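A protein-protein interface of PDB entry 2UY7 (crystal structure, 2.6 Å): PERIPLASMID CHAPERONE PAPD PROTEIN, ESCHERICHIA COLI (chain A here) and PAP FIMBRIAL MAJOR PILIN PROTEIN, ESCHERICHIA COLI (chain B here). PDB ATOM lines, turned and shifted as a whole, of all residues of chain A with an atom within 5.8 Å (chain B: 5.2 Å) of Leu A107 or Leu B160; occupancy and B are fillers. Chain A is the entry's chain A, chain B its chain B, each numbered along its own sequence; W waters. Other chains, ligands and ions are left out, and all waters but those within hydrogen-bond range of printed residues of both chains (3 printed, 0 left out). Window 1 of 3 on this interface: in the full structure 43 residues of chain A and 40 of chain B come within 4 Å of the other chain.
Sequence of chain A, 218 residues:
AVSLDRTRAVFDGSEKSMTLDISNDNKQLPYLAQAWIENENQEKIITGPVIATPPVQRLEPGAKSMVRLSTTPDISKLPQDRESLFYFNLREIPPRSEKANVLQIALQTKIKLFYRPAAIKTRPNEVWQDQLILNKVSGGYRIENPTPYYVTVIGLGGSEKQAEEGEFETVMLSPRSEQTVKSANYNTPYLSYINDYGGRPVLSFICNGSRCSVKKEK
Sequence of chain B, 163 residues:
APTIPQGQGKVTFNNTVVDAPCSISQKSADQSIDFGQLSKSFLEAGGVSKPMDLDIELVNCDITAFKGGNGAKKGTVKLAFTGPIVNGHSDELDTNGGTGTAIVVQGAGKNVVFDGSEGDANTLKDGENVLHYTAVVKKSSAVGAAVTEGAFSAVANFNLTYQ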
ATOM      1  N   ALA A   1     -11.022  -3.246 -21.962  1.00  0.00           N
ATOM      2  CA  ALA A   1     -10.477  -4.327 -21.089  1.00  0.00           C
ATOM      3  C   ALA A   1     -11.431  -5.529 -21.035  1.00  0.00           C
ATOM      4  O   ALA A   1     -11.001  -6.671 -21.191  1.00  0.00           O
ATOM      5  CB  ALA A   1     -10.224  -3.785 -19.676  1.00  0.00           C
ATOM      6  N   VAL A   2     -12.719  -5.271 -20.812  1.00  0.00           N
ATOM      7  CA  VAL A   2     -13.708  -6.341 -20.751  1.00  0.00           C
ATOM      8  C   VAL A   2     -14.088  -6.795 -22.144  1.00  0.00           C
ATOM      9  O   VAL A   2     -14.270  -5.975 -23.030  1.00  0.00           O
ATOM     10  CB  VAL A   2     -15.012  -5.895 -20.067  1.00  0.00           C
ATOM     11  CG1 VAL A   2     -15.995  -7.061 -20.035  1.00  0.00           C
ATOM     12  CG2 VAL A   2     -14.728  -5.407 -18.667  1.00  0.00           C
ATOM     13  N   LEU A  90     -22.759  -5.588 -23.424  1.00  0.00           N
ATOM     14  CA  LEU A  90     -21.705  -5.728 -22.437  1.00  0.00           C
ATOM     15  C   LEU A  90     -20.903  -4.447 -22.402  1.00  0.00           C
ATOM     16  O   LEU A  90     -20.132  -4.189 -23.313  1.00  0.00           O
ATOM     17  CB  LEU A  90     -20.780  -6.885 -22.810  1.00  0.00           C
ATOM     18  CG  LEU A  90     -19.776  -7.245 -21.719  1.00  0.00           C
ATOM     19  CD1 LEU A  90     -20.528  -7.790 -20.483  1.00  0.00           C
ATOM     20  CD2 LEU A  90     -18.793  -8.281 -22.273  1.00  0.00           C
ATOM     21  N   ARG A  91     -21.086  -3.644 -21.359  1.00  0.00           N
ATOM     22  CA  ARG A  91     -20.353  -2.388 -21.246  1.00  0.00           C
ATOM     23  C   ARG A  91     -19.465  -2.379 -20.010  1.00  0.00           C
ATOM     24  O   ARG A  91     -19.904  -2.722 -18.915  1.00  0.00           O
ATOM     25  CB  ARG A  91     -21.327  -1.208 -21.193  1.00  0.00           C
ATOM     26  CG  ARG A  91     -20.646   0.118 -20.911  1.00  0.00           C
ATOM     27  CD  ARG A  91     -21.635   1.151 -20.412  1.00  0.00           C
ATOM     28  NE  ARG A  91     -22.590   1.516 -21.450  1.00  0.00           N
ATOM     29  CZ  ARG A  91     -23.795   2.019 -21.205  1.00  0.00           C
ATOM     30  NH1 ARG A  91     -24.593   2.322 -22.213  1.00  0.00           N
ATOM     31  NH2 ARG A  91     -24.208   2.203 -19.953  1.00  0.00           N
ATOM     32  N   GLU A  92     -18.214  -1.981 -20.190  1.00  0.00           N
ATOM     33  CA  GLU A  92     -17.268  -1.926 -19.089  1.00  0.00           C
ATOM     34  C   GLU A  92     -17.284  -0.556 -18.422  1.00  0.00           C
ATOM     35  O   GLU A  92     -17.652   0.442 -19.039  1.00  0.00           O
ATOM     36  CB  GLU A  92     -15.849  -2.219 -19.590  1.00  0.00           C
ATOM     37  CG  GLU A  92     -15.218  -1.106 -20.416  1.00  0.00           C
ATOM     38  CD  GLU A  92     -13.852  -1.492 -20.989  1.00  0.00           C
ATOM     39  OE1 GLU A  92     -13.272  -0.697 -21.766  1.00  0.00           O
ATOM     40  OE2 GLU A  92     -13.353  -2.590 -20.665  1.00  0.00           O
ATOM     41  N   ILE A 105     -11.664   5.988 -22.038  1.00  0.00           N
ATOM     42  CA  ILE A 105     -12.469   5.282 -23.022  1.00  0.00           C
ATOM     43  C   ILE A 105     -13.061   4.044 -22.365  1.00  0.00           C
ATOM     44  O   ILE A 105     -12.367   3.347 -21.624  1.00  0.00           O
ATOM     45  CB  ILE A 105     -11.603   4.827 -24.217  1.00  0.00           C
ATOM     46  CG1 ILE A 105     -11.072   6.050 -24.962  1.00  0.00           C
ATOM     47  CG2 ILE A 105     -12.399   3.928 -25.130  1.00  0.00           C
ATOM     48  CD1 ILE A 105     -12.153   7.000 -25.410  1.00  0.00           C
ATOM     49  N   ALA A 106     -14.333   3.773 -22.630  1.00  0.00           N
ATOM     50  CA  ALA A 106     -14.999   2.602 -22.069  1.00  0.00           C
ATOM     51  C   ALA A 106     -15.642   1.834 -23.217  1.00  0.00           C
ATOM     52  O   ALA A 106     -16.499   2.367 -23.923  1.00  0.00           O
ATOM     53  CB  ALA A 106     -16.060   3.033 -21.057  1.00  0.00           C
ATOM     54  N   LEU A 107     -15.237   0.582 -23.413  1.00  0.00           N
ATOM     55  CA  LEU A 107     -15.798  -0.210 -24.498  1.00  0.00           C
ATOM     56  C   LEU A 107     -17.164  -0.794 -24.170  1.00  0.00           C
ATOM     57  O   LEU A 107     -17.466  -1.126 -23.019  1.00  0.00           O
ATOM     58  CB  LEU A 107     -14.830  -1.332 -24.886  1.00  0.00           C
ATOM     59  CG  LEU A 107     -15.126  -2.274 -26.069  1.00  0.00           C
ATOM     60  CD1 LEU A 107     -16.146  -3.289 -25.684  1.00  0.00           C
ATOM     61  CD2 LEU A 107     -15.596  -1.494 -27.271  1.00  0.00           C
ATOM     62  N   GLN A 108     -17.995  -0.885 -25.203  1.00  0.00           N
ATOM     63  CA  GLN A 108     -19.329  -1.464 -25.099  1.00  0.00           C
ATOM     64  C   GLN A 108     -19.509  -2.356 -26.316  1.00  0.00           C
ATOM     65  O   GLN A 108     -19.395  -1.896 -27.449  1.00  0.00           O
ATOM     66  CB  GLN A 108     -20.427  -0.398 -25.104  1.00  0.00           C
ATOM     67  CG  GLN A 108     -21.826  -1.010 -24.986  1.00  0.00           C
ATOM     68  CD  GLN A 108     -22.955   0.012 -25.034  1.00  0.00           C
ATOM     69  OE1 GLN A 108     -22.925   1.027 -24.338  1.00  0.00           O
ATOM     70  NE2 GLN A 108     -23.971  -0.269 -25.843  1.00  0.00           N
ATOM     71  N   THR A 109     -19.776  -3.633 -26.075  1.00  0.00           N
ATOM     72  CA  THR A 109     -19.984  -4.593 -27.146  1.00  0.00           C
ATOM     73  C   THR A 109     -21.468  -4.905 -27.246  1.00  0.00           C
ATOM     74  O   THR A 109     -22.121  -5.158 -26.235  1.00  0.00           O
ATOM     75  CB  THR A 109     -19.232  -5.915 -26.868  1.00  0.00           C
ATOM     76  OG1 THR A 109     -17.827  -5.662 -26.762  1.00  0.00           O
ATOM     77  CG2 THR A 109     -19.476  -6.914 -27.991  1.00  0.00           C
ATOM     78  N   LYS A 110     -22.004  -4.882 -28.464  1.00  0.00           N
ATOM     79  CA  LYS A 110     -23.413  -5.186 -28.681  1.00  0.00           C
ATOM     80  C   LYS A 110     -23.531  -6.231 -29.782  1.00  0.00           C
ATOM     81  O   LYS A 110     -23.078  -6.016 -30.903  1.00  0.00           O
ATOM     82  CB  LYS A 110     -24.204  -3.930 -29.075  1.00  0.00           C
ATOM     83  CG  LYS A 110     -25.692  -4.212 -29.268  1.00  0.00           C
ATOM     84  CD  LYS A 110     -26.407  -3.162 -30.100  1.00  0.00           C
ATOM     85  CE  LYS A 110     -27.164  -2.151 -29.252  1.00  0.00           C
ATOM     86  NZ  LYS A 110     -26.241  -1.248 -28.520  1.00  0.00           N
ATOM     87  N   ILE A 111     -24.121  -7.377 -29.468  1.00  0.00           N
ATOM     88  CA  ILE A 111     -24.259  -8.416 -30.478  1.00  0.00           C
ATOM     89  C   ILE A 111     -25.704  -8.823 -30.609  1.00  0.00           C
ATOM     90  O   ILE A 111     -26.552  -8.452 -29.802  1.00  0.00           O
ATOM     91  CB  ILE A 111     -23.428  -9.686 -30.146  1.00  0.00           C
ATOM     92  CG1 ILE A 111     -23.929 -10.318 -28.847  1.00  0.00           C
ATOM     93  CG2 ILE A 111     -21.943  -9.336 -30.030  1.00  0.00           C
ATOM     94  CD1 ILE A 111     -23.446 -11.736 -28.635  1.00  0.00           C
ATOM     95  N   CYS B  22     -14.152  -7.586 -30.636  1.00  0.00           N
ATOM     96  CA  CYS B  22     -12.877  -7.005 -30.257  1.00  0.00           C
ATOM     97  C   CYS B  22     -12.789  -6.686 -28.777  1.00  0.00           C
ATOM     98  O   CYS B  22     -13.794  -6.561 -28.085  1.00  0.00           O
ATOM     99  CB  CYS B  22     -12.600  -5.724 -31.035  1.00  0.00           C
ATOM    100  SG  CYS B  22     -12.574  -5.926 -32.842  1.00  0.00           S
ATOM    101  N   ILE B  24     -10.506  -3.931 -26.442  1.00  0.00           N
ATOM    102  CA  ILE B  24      -9.648  -2.766 -26.638  1.00  0.00           C
ATOM    103  C   ILE B  24      -8.692  -2.557 -25.485  1.00  0.00           C
ATOM    104  O   ILE B  24      -8.931  -3.007 -24.377  1.00  0.00           O
ATOM    105  CB  ILE B  24     -10.467  -1.448 -26.780  1.00  0.00           C
ATOM    106  CG1 ILE B  24     -11.161  -1.144 -25.453  1.00  0.00           C
ATOM    107  CG2 ILE B  24     -11.467  -1.554 -27.913  1.00  0.00           C
ATOM    108  CD1 ILE B  24     -11.824   0.193 -25.377  1.00  0.00           C
ATOM    109  N   GLN B  31      -7.059   3.003 -19.388  1.00  0.00           N
ATOM    110  CA  GLN B  31      -7.622   3.454 -20.649  1.00  0.00           C
ATOM    111  C   GLN B  31      -7.895   4.957 -20.660  1.00  0.00           C
ATOM    112  O   GLN B  31      -9.006   5.417 -20.951  1.00  0.00           O
ATOM    113  CB  GLN B  31      -8.887   2.651 -20.954  1.00  0.00           C
ATOM    114  CG  GLN B  31      -8.549   1.244 -21.415  1.00  0.00           C
ATOM    115  CD  GLN B  31      -9.751   0.334 -21.579  1.00  0.00           C
ATOM    116  OE1 GLN B  31     -10.897   0.790 -21.653  1.00  0.00           O
ATOM    117  NE2 GLN B  31      -9.491  -0.971 -21.652  1.00  0.00           N
ATOM    118  N   LEU B  58      -7.016  -3.026 -31.034  1.00  0.00           N
ATOM    119  CA  LEU B  58      -8.089  -4.000 -31.149  1.00  0.00           C
ATOM    120  C   LEU B  58      -7.486  -5.397 -31.120  1.00  0.00           C
ATOM    121  O   LEU B  58      -6.753  -5.773 -32.038  1.00  0.00           O
ATOM    122  CB  LEU B  58      -8.849  -3.801 -32.463  1.00  0.00           C
ATOM    123  CG  LEU B  58      -9.436  -2.418 -32.721  1.00  0.00           C
ATOM    124  CD1 LEU B  58      -9.992  -2.370 -34.127  1.00  0.00           C
ATOM    125  CD2 LEU B  58     -10.522  -2.112 -31.700  1.00  0.00           C
ATOM    126  N   PHE B  66     -12.487  -3.262 -39.818  1.00  0.00           N
ATOM    127  CA  PHE B  66     -12.342  -1.869 -39.406  1.00  0.00           C
ATOM    128  C   PHE B  66     -11.463  -1.195 -40.448  1.00  0.00           C
ATOM    129  O   PHE B  66     -10.260  -1.025 -40.234  1.00  0.00           O
ATOM    130  CB  PHE B  66     -11.663  -1.762 -38.037  1.00  0.00           C
ATOM    131  CG  PHE B  66     -12.474  -2.314 -36.914  1.00  0.00           C
ATOM    132  CD1 PHE B  66     -12.537  -3.683 -36.697  1.00  0.00           C
ATOM    133  CD2 PHE B  66     -13.177  -1.464 -36.072  1.00  0.00           C
ATOM    134  CE1 PHE B  66     -13.293  -4.197 -35.654  1.00  0.00           C
ATOM    135  CE2 PHE B  66     -13.934  -1.968 -35.029  1.00  0.00           C
ATOM    136  CZ  PHE B  66     -13.993  -3.337 -34.816  1.00  0.00           C
ATOM    137  N   VAL B  77     -18.986  -4.462 -38.763  1.00  0.00           N
ATOM    138  CA  VAL B  77     -18.998  -3.918 -37.409  1.00  0.00           C
ATOM    139  C   VAL B  77     -19.179  -2.405 -37.455  1.00  0.00           C
ATOM    140  O   VAL B  77     -18.438  -1.712 -38.148  1.00  0.00           O
ATOM    141  CB  VAL B  77     -17.664  -4.195 -36.677  1.00  0.00           C
ATOM    142  CG1 VAL B  77     -17.706  -3.590 -35.282  1.00  0.00           C
ATOM    143  CG2 VAL B  77     -17.403  -5.687 -36.604  1.00  0.00           C
ATOM    144  N   LYS B  78     -20.154  -1.897 -36.710  1.00  0.00           N
ATOM    145  CA  LYS B  78     -20.409  -0.467 -36.671  1.00  0.00           C
ATOM    146  C   LYS B  78     -19.716   0.121 -35.444  1.00  0.00           C
ATOM    147  O   LYS B  78     -19.814  -0.416 -34.346  1.00  0.00           O
ATOM    148  CB  LYS B  78     -21.914  -0.197 -36.626  1.00  0.00           C
ATOM    149  N   LEU B  79     -19.011   1.227 -35.646  1.00  0.00           N
ATOM    150  CA  LEU B  79     -18.265   1.911 -34.594  1.00  0.00           C
ATOM    151  C   LEU B  79     -18.990   3.213 -34.217  1.00  0.00           C
ATOM    152  O   LEU B  79     -19.606   3.835 -35.063  1.00  0.00           O
ATOM    153  CB  LEU B  79     -16.870   2.190 -35.139  1.00  0.00           C
ATOM    154  CG  LEU B  79     -15.767   2.849 -34.335  1.00  0.00           C
ATOM    155  CD1 LEU B  79     -14.466   2.700 -35.113  1.00  0.00           C
ATOM    156  CD2 LEU B  79     -16.090   4.305 -34.090  1.00  0.00           C
ATOM    157  N   PHE B 158     -16.983   3.909 -26.259  1.00  0.00           N
ATOM    158  CA  PHE B 158     -16.594   3.455 -27.588  1.00  0.00           C
ATOM    159  C   PHE B 158     -17.480   2.238 -27.824  1.00  0.00           C
ATOM    160  O   PHE B 158     -17.270   1.181 -27.230  1.00  0.00           O
ATOM    161  CB  PHE B 158     -15.111   3.074 -27.604  1.00  0.00           C
ATOM    162  CG  PHE B 158     -14.609   2.627 -28.948  1.00  0.00           C
ATOM    163  CD1 PHE B 158     -14.642   3.485 -30.039  1.00  0.00           C
ATOM    164  CD2 PHE B 158     -14.098   1.341 -29.121  1.00  0.00           C
ATOM    165  CE1 PHE B 158     -14.171   3.071 -31.285  1.00  0.00           C
ATOM    166  CE2 PHE B 158     -13.626   0.918 -30.361  1.00  0.00           C
ATOM    167  CZ  PHE B 158     -13.662   1.782 -31.444  1.00  0.00           C
ATOM    168  N   ASN B 159     -18.480   2.398 -28.684  1.00  0.00           N
ATOM    169  CA  ASN B 159     -19.437   1.336 -28.967  1.00  0.00           C
ATOM    170  C   ASN B 159     -19.188   0.553 -30.257  1.00  0.00           C
ATOM    171  O   ASN B 159     -19.121   1.124 -31.345  1.00  0.00           O
ATOM    172  CB  ASN B 159     -20.855   1.926 -29.011  1.00  0.00           C
ATOM    173  CG  ASN B 159     -21.136   2.892 -27.849  1.00  0.00           C
ATOM    174  OD1 ASN B 159     -21.281   2.473 -26.688  1.00  0.00           O
ATOM    175  ND2 ASN B 159     -21.211   4.194 -28.160  1.00  0.00           N
ATOM    176  N   LEU B 160     -19.056  -0.763 -30.125  1.00  0.00           N
ATOM    177  CA  LEU B 160     -18.867  -1.636 -31.273  1.00  0.00           C
ATOM    178  C   LEU B 160     -20.104  -2.542 -31.350  1.00  0.00           C
ATOM    179  O   LEU B 160     -20.417  -3.256 -30.408  1.00  0.00           O
ATOM    180  CB  LEU B 160     -17.582  -2.464 -31.121  1.00  0.00           C
ATOM    181  CG  LEU B 160     -16.262  -1.668 -31.118  1.00  0.00           C
ATOM    182  CD1 LEU B 160     -15.070  -2.616 -31.075  1.00  0.00           C
ATOM    183  CD2 LEU B 160     -16.182  -0.786 -32.367  1.00  0.00           C
ATOM    184  N   THR B 161     -20.819  -2.490 -32.469  1.00  0.00           N
ATOM    185  CA  THR B 161     -22.027  -3.292 -32.662  1.00  0.00           C
ATOM    186  C   THR B 161     -21.763  -4.243 -33.815  1.00  0.00           C
ATOM    187  O   THR B 161     -21.347  -3.809 -34.885  1.00  0.00           O
ATOM    188  CB  THR B 161     -23.242  -2.398 -33.000  1.00  0.00           C
ATOM    189  OG1 THR B 161     -23.385  -1.393 -31.992  1.00  0.00           O
ATOM    190  CG2 THR B 161     -24.510  -3.218 -33.035  1.00  0.00           C
ATOM    191  N   TYR B 162     -22.011  -5.534 -33.607  1.00  0.00           N
ATOM    192  CA  TYR B 162     -21.716  -6.527 -34.636  1.00  0.00           C
ATOM    193  C   TYR B 162     -22.913  -7.039 -35.389  1.00  0.00           C
ATOM    194  O   TYR B 162     -23.945  -7.378 -34.811  1.00  0.00           O
ATOM    195  CB  TYR B 162     -20.963  -7.719 -34.032  1.00  0.00           C
ATOM    196  CG  TYR B 162     -19.666  -7.332 -33.360  1.00  0.00           C
ATOM    197  CD1 TYR B 162     -19.669  -6.566 -32.191  1.00  0.00           C
ATOM    198  CD2 TYR B 162     -18.437  -7.656 -33.936  1.00  0.00           C
ATOM    199  CE1 TYR B 162     -18.489  -6.123 -31.624  1.00  0.00           C
ATOM    200  CE2 TYR B 162     -17.242  -7.219 -33.373  1.00  0.00           C
ATOM    201  CZ  TYR B 162     -17.279  -6.448 -32.221  1.00  0.00           C
ATOM    202  OH  TYR B 162     -16.109  -5.972 -31.683  1.00  0.00           O
HETATM  203  O   HOH W   1     -15.757  -8.122 -26.814  1.00  0.00           O
HETATM  204  O   HOH W   2     -11.771  -4.651 -24.026  1.00  0.00           O
HETATM  205  O   HOH W   3     -16.211  -5.399 -29.072  1.00  0.00           O
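The side-chain carboxylate (OE1) of Glu A92 lies close to the side-chain amide oxygen (OE1) of Gln B31, 2.8 Å away.
The backbone carbonyl oxygen (O) of Ala A106 is in hydrogen-bond range of the backbone NH (N) of Phe B158, 2.8 Å away.
N of Ala A1 is in hydrogen-bond range of O of Ile B24, 3.2 Å away.
The backbone carbonyl oxygen (O) of Leu B160 is in hydrogen-bond range of the backbone NH (N) of Lys A110, at 3.0 Å.
The backbone NH (N) of Tyr B162 is in hydrogen-bond range of the backbone carbonyl oxygen (O) of Lys A110, 2.9 Å away.
The backbone NH (N) of Ile A105 sits at hydrogen-bond distance from the backbone carbonyl oxygen (O) of Gln B31.
O of Gln A108 sits at hydrogen-bond distance from N of Leu B160, at 2.9 Å.
The backbone NH (N) of Ala A1 lies close to the side-chain amide nitrogen (NE2) of Gln B31, at 2.8 Å.
The backbone NH (N) of Gln A108 is in hydrogen-bond range of the backbone carbonyl oxygen (O) of Phe B158.
OE1 of Gln A108 sits close to OD1 of Asn B159 (3.2 Å).
The backbone NH of Cys B22 is in hydrogen-bond range of the side-chain hydroxyl of Tyr B162, at 2.7 Å.
The backbone carbonyl oxygen (O) of Ile B24 sits at hydrogen-bond distance from the side-chain amide nitrogen (NE2) of Gln B31, 3.4 Å away.
The backbone NH (N) of Thr A109 is in hydrogen-bond range of the backbone carbonyl oxygen (O) of Leu A90 (2.8 Å).
NE of Arg A91 sits at hydrogen-bond distance from OE1 of Gln A108 (2.9 Å).
The side-chain carboxylate of Glu A92 sits at hydrogen-bond distance from the backbone NH of Ala A1.
The side-chain carboxylate of Glu A92 lies within hydrogen-bond range of the backbone NH of Leu A107 (2.9 Å).
Among the printed residues, merely in contact across the chains: Glu A92 with Ile B24 (3.99 Å), Ile A105 with Ile B24 (3.8 Å), Ile A105 with Phe B158 (3.8 Å), Leu A107 with Ile B24 (3.4 Å), Leu A107 with Phe B158 (3.2 Å), Leu A107 with Leu B160 (3.9 Å), Thr A109 with Leu B160 (3.6 Å), Thr A109 with Tyr B162 (3.8 Å) and Lys A110 with Thr B161 (3.4 Å).
Arg A91 touches none of the printed residues of chain B.
Of the printed residues of chain B, Ile A105 touches Ile B24 (3.8 Å), Gln B31 (2.9 Å) and Phe B158 (3.8 Å).
Leu A107 touches three residues of chain B.
Leu B79 touches none of the printed residues of chain A.
Of the printed residues of chain A, Asn B159 touches Gln A108 (3.2 Å).
Leu B160 touches just these residues of chain A: Leu A107, Gln A108, Thr A109 and Lys A110.
Of the printed residues of chain A, Thr B161 touches Lys A110.
The nearest printed residue of chain B that does not touch Leu A107 is Gln B31 (4.7 Å).
Of the 12 printed residues of chain A, 8 touch a printed residue of chain B.
Printed residues of chain A that touch a printed residue of chain B: Ala A1, Glu A92, Ile A105, Ala A106, Leu A107, Gln A108, Thr A109 and Lys A110.
Hydrophobic or aromatic side chains of chain A within 4 Å of the printed part of chain B: Ala A1, Ile A105 and Leu A107.
Of the 13 printed residues of chain B, 7 touch a printed residue of chain A.
Printed residues of chain B that touch a printed residue of chain A: Ile B24, Gln B31, Phe B158, Asn B159, Leu B160, Thr B161 and Tyr B162.
Water W2 lies within hydrogen-bond range of the backbone NH (N) of Ala A1, the backbone NH (N) of Ile B24 and the backbone carbonyl oxygen (O) of Val A2.
Water W3 lies within hydrogen-bond range of OH of Tyr B162 (2.7 Å), OG1 of Thr A109 (2.8 Å) and O of Cys B22 (2.9 Å).
Water W1 lies within hydrogen-bond range of the backbone carbonyl oxygen of Cys B22 (2.8 Å) and the side-chain hydroxyl of Thr A109 (3.2 Å).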
